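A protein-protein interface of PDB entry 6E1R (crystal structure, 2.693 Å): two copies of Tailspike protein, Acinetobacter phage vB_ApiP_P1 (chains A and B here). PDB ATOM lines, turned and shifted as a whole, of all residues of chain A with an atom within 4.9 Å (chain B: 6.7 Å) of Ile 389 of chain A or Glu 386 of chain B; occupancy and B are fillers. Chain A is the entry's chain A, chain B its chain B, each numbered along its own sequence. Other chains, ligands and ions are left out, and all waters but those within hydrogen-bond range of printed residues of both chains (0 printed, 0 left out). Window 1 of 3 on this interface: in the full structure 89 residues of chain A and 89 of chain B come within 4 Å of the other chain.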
ATOM      1  N   PHE A 360     -15.544   1.995  24.206  1.00  0.00           N
ATOM      2  CA  PHE A 360     -16.404   2.356  23.084  1.00  0.00           C
ATOM      3  C   PHE A 360     -15.857   3.662  22.522  1.00  0.00           C
ATOM      4  O   PHE A 360     -16.054   4.732  23.106  1.00  0.00           O
ATOM      5  CB  PHE A 360     -17.861   2.486  23.518  1.00  0.00           C
ATOM      6  CG  PHE A 360     -18.503   1.179  23.888  1.00  0.00           C
ATOM      7  CD1 PHE A 360     -18.332   0.638  25.153  1.00  0.00           C
ATOM      8  CD2 PHE A 360     -19.286   0.496  22.972  1.00  0.00           C
ATOM      9  CE1 PHE A 360     -18.924  -0.566  25.493  1.00  0.00           C
ATOM     10  CE2 PHE A 360     -19.883  -0.707  23.306  1.00  0.00           C
ATOM     11  CZ  PHE A 360     -19.701  -1.237  24.569  1.00  0.00           C
ATOM     12  N   GLU A 361     -15.167   3.567  21.390  1.00  0.00           N
ATOM     13  CA  GLU A 361     -14.435   4.685  20.804  1.00  0.00           C
ATOM     14  C   GLU A 361     -15.096   5.067  19.484  1.00  0.00           C
ATOM     15  O   GLU A 361     -14.920   4.385  18.471  1.00  0.00           O
ATOM     16  CB  GLU A 361     -12.970   4.310  20.614  1.00  0.00           C
ATOM     17  CG  GLU A 361     -12.063   5.460  20.233  1.00  0.00           C
ATOM     18  CD  GLU A 361     -10.638   5.003  20.009  1.00  0.00           C
ATOM     19  OE1 GLU A 361      -9.910   4.806  21.006  1.00  0.00           O
ATOM     20  OE2 GLU A 361     -10.251   4.819  18.839  1.00  0.00           O
ATOM     21  N   GLY A 362     -15.854   6.161  19.503  1.00  0.00           N
ATOM     22  CA  GLY A 362     -16.455   6.682  18.293  1.00  0.00           C
ATOM     23  C   GLY A 362     -17.566   5.844  17.705  1.00  0.00           C
ATOM     24  O   GLY A 362     -17.878   6.000  16.522  1.00  0.00           O
ATOM     25  N   ASN A 387     -13.091   3.287  28.901  1.00  0.00           N
ATOM     26  CA  ASN A 387     -13.157   4.574  28.221  1.00  0.00           C
ATOM     27  C   ASN A 387     -14.376   4.592  27.312  1.00  0.00           C
ATOM     28  O   ASN A 387     -14.762   3.562  26.752  1.00  0.00           O
ATOM     29  CB  ASN A 387     -11.883   4.854  27.415  1.00  0.00           C
ATOM     30  CG  ASN A 387     -11.638   6.333  27.211  1.00  0.00           C
ATOM     31  OD1 ASN A 387     -11.728   6.838  26.093  1.00  0.00           O
ATOM     32  ND2 ASN A 387     -11.339   7.042  28.295  1.00  0.00           N
ATOM     33  N   SER A 388     -14.975   5.776  27.174  1.00  0.00           N
ATOM     34  CA  SER A 388     -16.156   5.957  26.328  1.00  0.00           C
ATOM     35  C   SER A 388     -16.095   7.376  25.771  1.00  0.00           C
ATOM     36  O   SER A 388     -16.490   8.327  26.451  1.00  0.00           O
ATOM     37  CB  SER A 388     -17.438   5.717  27.113  1.00  0.00           C
ATOM     38  OG  SER A 388     -18.565   6.229  26.422  1.00  0.00           O
ATOM     39  N   ILE A 389     -15.602   7.510  24.540  1.00  0.00           N
ATOM     40  CA  ILE A 389     -15.337   8.812  23.940  1.00  0.00           C
ATOM     41  C   ILE A 389     -15.965   8.881  22.555  1.00  0.00           C
ATOM     42  O   ILE A 389     -15.929   7.909  21.793  1.00  0.00           O
ATOM     43  CB  ILE A 389     -13.824   9.103  23.862  1.00  0.00           C
ATOM     44  CG1 ILE A 389     -13.074   7.902  23.280  1.00  0.00           C
ATOM     45  CG2 ILE A 389     -13.282   9.482  25.234  1.00  0.00           C
ATOM     46  CD1 ILE A 389     -11.590   8.142  23.092  1.00  0.00           C
ATOM     47  N   ALA A 390     -16.549  10.041  22.240  1.00  0.00           N
ATOM     48  CA  ALA A 390     -17.058  10.358  20.905  1.00  0.00           C
ATOM     49  C   ALA A 390     -18.110   9.361  20.427  1.00  0.00           C
ATOM     50  O   ALA A 390     -18.275   9.145  19.226  1.00  0.00           O
ATOM     51  CB  ALA A 390     -15.917  10.456  19.889  1.00  0.00           C
ATOM     52  N   ASN A 391     -18.841   8.758  21.359  1.00  0.00           N
ATOM     53  CA  ASN A 391     -19.909   7.831  21.016  1.00  0.00           C
ATOM     54  C   ASN A 391     -21.220   8.581  20.819  1.00  0.00           C
ATOM     55  O   ASN A 391     -21.518   9.535  21.541  1.00  0.00           O
ATOM     56  CB  ASN A 391     -20.080   6.777  22.110  1.00  0.00           C
ATOM     57  CG  ASN A 391     -18.855   5.907  22.276  1.00  0.00           C
ATOM     58  OD1 ASN A 391     -18.326   5.367  21.305  1.00  0.00           O
ATOM     59  ND2 ASN A 391     -18.392   5.769  23.515  1.00  0.00           N
ATOM     60  N   LEU A 407     -22.134  11.698  23.181  1.00  0.00           N
ATOM     61  CA  LEU A 407     -22.097  13.042  22.611  1.00  0.00           C
ATOM     62  C   LEU A 407     -23.350  13.833  22.968  1.00  0.00           C
ATOM     63  O   LEU A 407     -23.282  15.047  23.196  1.00  0.00           O
ATOM     64  CB  LEU A 407     -21.924  12.963  21.095  1.00  0.00           C
ATOM     65  CG  LEU A 407     -20.548  12.519  20.593  1.00  0.00           C
ATOM     66  CD1 LEU A 407     -20.515  12.485  19.073  1.00  0.00           C
ATOM     67  CD2 LEU A 407     -19.461  13.432  21.135  1.00  0.00           C
ATOM     68  N   ASN A 414     -16.712   9.532  31.070  1.00  0.00           N
ATOM     69  CA  ASN A 414     -15.932   8.893  30.017  1.00  0.00           C
ATOM     70  C   ASN A 414     -15.322   7.585  30.499  1.00  0.00           C
ATOM     71  O   ASN A 414     -15.165   6.646  29.709  1.00  0.00           O
ATOM     72  CB  ASN A 414     -14.834   9.833  29.520  1.00  0.00           C
ATOM     73  CG  ASN A 414     -15.386  11.083  28.871  1.00  0.00           C
ATOM     74  OD1 ASN A 414     -15.471  12.136  29.501  1.00  0.00           O
ATOM     75  ND2 ASN A 414     -15.770  10.972  27.605  1.00  0.00           N
ATOM     76  N   PRO B 330     -19.439  10.919  14.166  1.00  0.00           N
ATOM     77  CA  PRO B 330     -19.169  11.246  15.571  1.00  0.00           C
ATOM     78  C   PRO B 330     -17.692  11.493  15.827  1.00  0.00           C
ATOM     79  O   PRO B 330     -17.330  12.316  16.674  1.00  0.00           O
ATOM     80  CB  PRO B 330     -19.668  10.006  16.319  1.00  0.00           C
ATOM     81  CG  PRO B 330     -19.493   8.898  15.342  1.00  0.00           C
ATOM     82  CD  PRO B 330     -19.767   9.495  13.983  1.00  0.00           C
ATOM     83  N   LEU B 331     -16.833  10.788  15.097  1.00  0.00           N
ATOM     84  CA  LEU B 331     -15.403  10.827  15.357  1.00  0.00           C
ATOM     85  C   LEU B 331     -14.635  10.625  14.061  1.00  0.00           C
ATOM     86  O   LEU B 331     -14.975   9.752  13.258  1.00  0.00           O
ATOM     87  CB  LEU B 331     -14.997   9.753  16.372  1.00  0.00           C
ATOM     88  CG  LEU B 331     -13.494   9.526  16.543  1.00  0.00           C
ATOM     89  CD1 LEU B 331     -12.837  10.778  17.093  1.00  0.00           C
ATOM     90  CD2 LEU B 331     -13.220   8.325  17.436  1.00  0.00           C
ATOM     91  N   LYS B 357     -16.002  15.175  16.213  1.00  0.00           N
ATOM     92  CA  LYS B 357     -14.841  15.334  17.074  1.00  0.00           C
ATOM     93  C   LYS B 357     -13.638  14.654  16.427  1.00  0.00           C
ATOM     94  O   LYS B 357     -13.776  13.804  15.544  1.00  0.00           O
ATOM     95  CB  LYS B 357     -15.102  14.743  18.461  1.00  0.00           C
ATOM     96  CG  LYS B 357     -16.378  15.238  19.123  1.00  0.00           C
ATOM     97  CD  LYS B 357     -16.370  16.748  19.290  1.00  0.00           C
ATOM     98  CE  LYS B 357     -17.583  17.220  20.078  1.00  0.00           C
ATOM     99  NZ  LYS B 357     -17.677  18.707  20.107  1.00  0.00           N
ATOM    100  N   TYR B 358     -12.447  15.038  16.876  1.00  0.00           N
ATOM    101  CA  TYR B 358     -11.212  14.567  16.267  1.00  0.00           C
ATOM    102  C   TYR B 358     -10.305  13.944  17.317  1.00  0.00           C
ATOM    103  O   TYR B 358     -10.238  14.419  18.454  1.00  0.00           O
ATOM    104  CB  TYR B 358     -10.485  15.714  15.556  1.00  0.00           C
ATOM    105  CG  TYR B 358     -11.230  16.240  14.349  1.00  0.00           C
ATOM    106  CD1 TYR B 358     -12.242  17.182  14.490  1.00  0.00           C
ATOM    107  CD2 TYR B 358     -10.923  15.796  13.071  1.00  0.00           C
ATOM    108  CE1 TYR B 358     -12.928  17.664  13.391  1.00  0.00           C
ATOM    109  CE2 TYR B 358     -11.603  16.272  11.965  1.00  0.00           C
ATOM    110  CZ  TYR B 358     -12.603  17.206  12.131  1.00  0.00           C
ATOM    111  OH  TYR B 358     -13.281  17.682  11.033  1.00  0.00           O
ATOM    112  N   ILE B 359      -9.615  12.874  16.927  1.00  0.00           N
ATOM    113  CA  ILE B 359      -8.577  12.251  17.741  1.00  0.00           C
ATOM    114  C   ILE B 359      -7.304  12.199  16.911  1.00  0.00           C
ATOM    115  O   ILE B 359      -7.297  11.638  15.808  1.00  0.00           O
ATOM    116  CB  ILE B 359      -8.974  10.845  18.214  1.00  0.00           C
ATOM    117  CG1 ILE B 359     -10.055  10.920  19.293  1.00  0.00           C
ATOM    118  CG2 ILE B 359      -7.756  10.107  18.751  1.00  0.00           C
ATOM    119  CD1 ILE B 359     -10.474   9.565  19.820  1.00  0.00           C
ATOM    120  N   PHE B 360      -6.234  12.789  17.433  1.00  0.00           N
ATOM    121  CA  PHE B 360      -4.908  12.725  16.823  1.00  0.00           C
ATOM    122  C   PHE B 360      -4.008  11.955  17.784  1.00  0.00           C
ATOM    123  O   PHE B 360      -3.591  12.488  18.816  1.00  0.00           O
ATOM    124  CB  PHE B 360      -4.372  14.123  16.530  1.00  0.00           C
ATOM    125  CG  PHE B 360      -5.117  14.840  15.441  1.00  0.00           C
ATOM    126  CD1 PHE B 360      -6.295  15.515  15.716  1.00  0.00           C
ATOM    127  CD2 PHE B 360      -4.641  14.838  14.139  1.00  0.00           C
ATOM    128  CE1 PHE B 360      -6.985  16.174  14.717  1.00  0.00           C
ATOM    129  CE2 PHE B 360      -5.324  15.497  13.135  1.00  0.00           C
ATOM    130  CZ  PHE B 360      -6.498  16.166  13.424  1.00  0.00           C
ATOM    131  N   VAL B 382     -10.678  23.727  20.438  1.00  0.00           N
ATOM    132  CA  VAL B 382     -10.416  22.612  21.341  1.00  0.00           C
ATOM    133  C   VAL B 382     -11.695  21.862  21.689  1.00  0.00           C
ATOM    134  O   VAL B 382     -11.639  20.692  22.084  1.00  0.00           O
ATOM    135  CB  VAL B 382      -9.695  23.117  22.606  1.00  0.00           C
ATOM    136  CG1 VAL B 382      -9.208  21.953  23.458  1.00  0.00           C
ATOM    137  CG2 VAL B 382      -8.526  24.010  22.219  1.00  0.00           C
ATOM    138  N   ALA B 383     -12.858  22.498  21.525  1.00  0.00           N
ATOM    139  CA  ALA B 383     -14.121  21.802  21.738  1.00  0.00           C
ATOM    140  C   ALA B 383     -14.336  20.680  20.729  1.00  0.00           C
ATOM    141  O   ALA B 383     -15.175  19.802  20.964  1.00  0.00           O
ATOM    142  CB  ALA B 383     -15.284  22.792  21.675  1.00  0.00           C
ATOM    143  N   LEU B 384     -13.605  20.688  19.616  1.00  0.00           N
ATOM    144  CA  LEU B 384     -13.693  19.635  18.613  1.00  0.00           C
ATOM    145  C   LEU B 384     -12.640  18.551  18.794  1.00  0.00           C
ATOM    146  O   LEU B 384     -12.639  17.576  18.035  1.00  0.00           O
ATOM    147  CB  LEU B 384     -13.567  20.230  17.207  1.00  0.00           C
ATOM    148  CG  LEU B 384     -14.567  21.316  16.811  1.00  0.00           C
ATOM    149  CD1 LEU B 384     -14.257  21.829  15.417  1.00  0.00           C
ATOM    150  CD2 LEU B 384     -15.988  20.783  16.883  1.00  0.00           C
ATOM    151  N   ILE B 385     -11.749  18.691  19.770  1.00  0.00           N
ATOM    152  CA  ILE B 385     -10.660  17.746  19.986  1.00  0.00           C
ATOM    153  C   ILE B 385     -11.113  16.765  21.061  1.00  0.00           C
ATOM    154  O   ILE B 385     -11.150  17.096  22.249  1.00  0.00           O
ATOM    155  CB  ILE B 385      -9.362  18.456  20.378  1.00  0.00           C
ATOM    156  CG1 ILE B 385      -8.936  19.429  19.276  1.00  0.00           C
ATOM    157  CG2 ILE B 385      -8.261  17.440  20.651  1.00  0.00           C
ATOM    158  CD1 ILE B 385      -8.798  18.789  17.912  1.00  0.00           C
ATOM    159  N   GLU B 386     -11.458  15.543  20.645  1.00  0.00           N
ATOM    160  CA  GLU B 386     -11.811  14.513  21.614  1.00  0.00           C
ATOM    161  C   GLU B 386     -10.581  14.003  22.355  1.00  0.00           C
ATOM    162  O   GLU B 386     -10.675  13.651  23.537  1.00  0.00           O
ATOM    163  CB  GLU B 386     -12.537  13.359  20.923  1.00  0.00           C
ATOM    164  CG  GLU B 386     -13.103  12.309  21.874  1.00  0.00           C
ATOM    165  CD  GLU B 386     -14.214  12.847  22.761  1.00  0.00           C
ATOM    166  OE1 GLU B 386     -14.932  13.773  22.327  1.00  0.00           O
ATOM    167  OE2 GLU B 386     -14.373  12.341  23.893  1.00  0.00           O
ATOM    168  N   ASN B 387      -9.430  13.962  21.688  1.00  0.00           N
ATOM    169  CA  ASN B 387      -8.181  13.572  22.329  1.00  0.00           C
ATOM    170  C   ASN B 387      -7.020  13.961  21.425  1.00  0.00           C
ATOM    171  O   ASN B 387      -7.135  13.934  20.198  1.00  0.00           O
ATOM    172  CB  ASN B 387      -8.138  12.068  22.628  1.00  0.00           C
ATOM    173  CG  ASN B 387      -7.210  11.734  23.780  1.00  0.00           C
ATOM    174  OD1 ASN B 387      -6.903  12.588  24.612  1.00  0.00           O
ATOM    175  ND2 ASN B 387      -6.762  10.486  23.836  1.00  0.00           N
ATOM    176  N   SER B 388      -5.902  14.324  22.055  1.00  0.00           N
ATOM    177  CA  SER B 388      -4.695  14.729  21.335  1.00  0.00           C
ATOM    178  C   SER B 388      -3.503  14.297  22.184  1.00  0.00           C
ATOM    179  O   SER B 388      -3.120  15.004  23.121  1.00  0.00           O
ATOM    180  CB  SER B 388      -4.689  16.231  21.078  1.00  0.00           C
ATOM    181  OG  SER B 388      -3.396  16.684  20.715  1.00  0.00           O
ATOM    182  N   ASN B 414      -5.040  18.219  26.160  1.00  0.00           N
ATOM    183  CA  ASN B 414      -5.224  16.958  25.451  1.00  0.00           C
ATOM    184  C   ASN B 414      -6.637  16.826  24.901  1.00  0.00           C
ATOM    185  O   ASN B 414      -6.838  16.210  23.849  1.00  0.00           O
ATOM    186  CB  ASN B 414      -4.912  15.778  26.374  1.00  0.00           C
ATOM    187  CG  ASN B 414      -3.464  15.749  26.814  1.00  0.00           C
ATOM    188  OD1 ASN B 414      -3.127  16.204  27.906  1.00  0.00           O
ATOM    189  ND2 ASN B 414      -2.599  15.200  25.968  1.00  0.00           N
ATOM    190  N   ALA B 415      -7.622  17.392  25.594  1.00  0.00           N
ATOM    191  CA  ALA B 415      -9.014  17.296  25.178  1.00  0.00           C
ATOM    192  C   ALA B 415      -9.782  18.459  25.786  1.00  0.00           C
ATOM    193  O   ALA B 415      -9.270  19.195  26.634  1.00  0.00           O
ATOM    194  CB  ALA B 415      -9.631  15.955  25.588  1.00  0.00           C
ATOM    195  N   ASP B 416     -11.028  18.616  25.338  1.00  0.00           N
ATOM    196  CA  ASP B 416     -11.875  19.679  25.869  1.00  0.00           C
ATOM    197  C   ASP B 416     -12.372  19.335  27.268  1.00  0.00           C
ATOM    198  O   ASP B 416     -12.300  20.164  28.184  1.00  0.00           O
ATOM    199  CB  ASP B 416     -13.049  19.936  24.924  1.00  0.00           C
ATOM    200  CG  ASP B 416     -13.991  21.005  25.443  1.00  0.00           C
ATOM    201  OD1 ASP B 416     -13.541  22.154  25.640  1.00  0.00           O
ATOM    202  OD2 ASP B 416     -15.184  20.698  25.652  1.00  0.00           O
ATOM    203  N   SER B 417     -12.876  18.116  27.456  1.00  0.00           N
ATOM    204  CA  SER B 417     -13.462  17.734  28.732  1.00  0.00           C
ATOM    205  C   SER B 417     -13.383  16.226  28.913  1.00  0.00           C
ATOM    206  O   SER B 417     -13.401  15.462  27.944  1.00  0.00           O
ATOM    207  CB  SER B 417     -14.918  18.201  28.843  1.00  0.00           C
ATOM    208  OG  SER B 417     -15.738  17.544  27.893  1.00  0.00           O
ATOM    209  N   ARG B 418     -13.299  15.810  30.176  1.00  0.00           N
ATOM    210  CA  ARG B 418     -13.346  14.409  30.572  1.00  0.00           C
ATOM    211  C   ARG B 418     -14.070  14.305  31.905  1.00  0.00           C
ATOM    212  O   ARG B 418     -13.864  15.135  32.792  1.00  0.00           O
ATOM    213  CB  ARG B 418     -11.944  13.799  30.694  1.00  0.00           C
ATOM    214  CG  ARG B 418     -11.297  13.434  29.374  1.00  0.00           C
ATOM    215  CD  ARG B 418     -12.080  12.347  28.655  1.00  0.00           C
ATOM    216  NE  ARG B 418     -11.342  11.823  27.510  1.00  0.00           N
ATOM    217  CZ  ARG B 418     -11.316  12.399  26.313  1.00  0.00           C
ATOM    218  NH1 ARG B 418     -11.990  13.520  26.099  1.00  0.00           N
ATOM    219  NH2 ARG B 418     -10.615  11.853  25.328  1.00  0.00           N
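Ile 389 of chain A touches three residues of chain B.
Glu 386 of chain B touches just these residues of chain A: Ile 389 and Ala 390.
Printed residues of chain B within 4 Å of Ala 390 of chain A: Pro 330 (3.3 Å), Leu 331 (3.7 Å) and Glu 386 (3.6 Å).
Of the printed residues of chain A, Ile 359 of chain B touches Ile 389.
Of the printed residues of chain B, Gly 362 of chain A touches Pro 330 and Leu 331.
Of the printed residues of chain A, Arg 418 of chain B touches Ile 389 and Asn 414.
Ala 415 of chain B touches none of the printed residues of chain A.
The nearest residue of chain B that does not touch Ile 389 of chain A is Leu 331 of chain B (5.1 Å).
The nearest residue of chain A that does not touch Glu 386 of chain B is Asn 414 of chain A (4.2 Å).
The nearest printed residue of chain B that does not touch Asn 414 of chain A is Glu 386 of chain B (4.2 Å).
The backbone carbonyl oxygen of Phe 360 of chain A sits at hydrogen-bond distance from the backbone NH of Ile 389 of chain A, 3.2 Å away.
The backbone NH of Gly 362 of chain A lies within hydrogen-bond range of the side-chain amide oxygen of Asn 391 of chain A, at 3.2 Å.
The backbone carbonyl oxygen (O) of Asn 414 of chain A is in hydrogen-bond range of the backbone NH (N) of Ser 388 of chain A (2.7 Å).
ND2 of Asn 391 of chain A sits close to N of Ile 389 of chain A.
The backbone NH (N) of Leu 407 of chain A sits at hydrogen-bond distance from the backbone carbonyl oxygen (O) of Asn 391 of chain A (2.8 Å).
The backbone NH (N) of Lys 357 of chain B sits at hydrogen-bond distance from the backbone carbonyl oxygen (O) of Pro 330 of chain B, at 3.2 Å.
Among the printed residues, pairs that only touch across the chains: Ile 389 of chain A with Glu 386 of chain B (3.3 Å), Asn 414 of chain A with Arg 418 of chain B (3.3 Å), Ala 390 of chain A with Pro 330 of chain B (3.3 Å), Gly 362 of chain A with Pro 330 of chain B (3.5 Å), Ile 389 of chain A with Arg 418 of chain B (3.6 Å), Ala 390 of chain A with Glu 386 of chain B (3.6 Å), Ala 390 of chain A with Leu 331 of chain B (3.7 Å), Gly 362 of chain A with Leu 331 of chain B (3.7 Å), Ile 389 of chain A with Ile 359 of chain B (3.7 Å) and Leu 407 of chain A with Pro 330 of chain B (3.8 Å).
Of the 10 printed residues of chain A, 5 touch a printed residue of chain B.
Printed residues of chain A that touch a printed residue of chain B: Gly 362, Ile 389, Ala 390, Leu 407 and Asn 414.
Of the 18 printed residues of chain B, 5 touch a printed residue of chain A.
Among the printed residues, 10 pairs touch across the chains.
Among the printed residues, no Asp or Glu carboxylate lies within 4 Å of a Lys or Arg side-chain nitrogen of the other chain.
4 positions are printed for both chains.
Of the 10 pairs that touch across the chains among the printed residues, none has its exchanged pair printed and touching as well.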
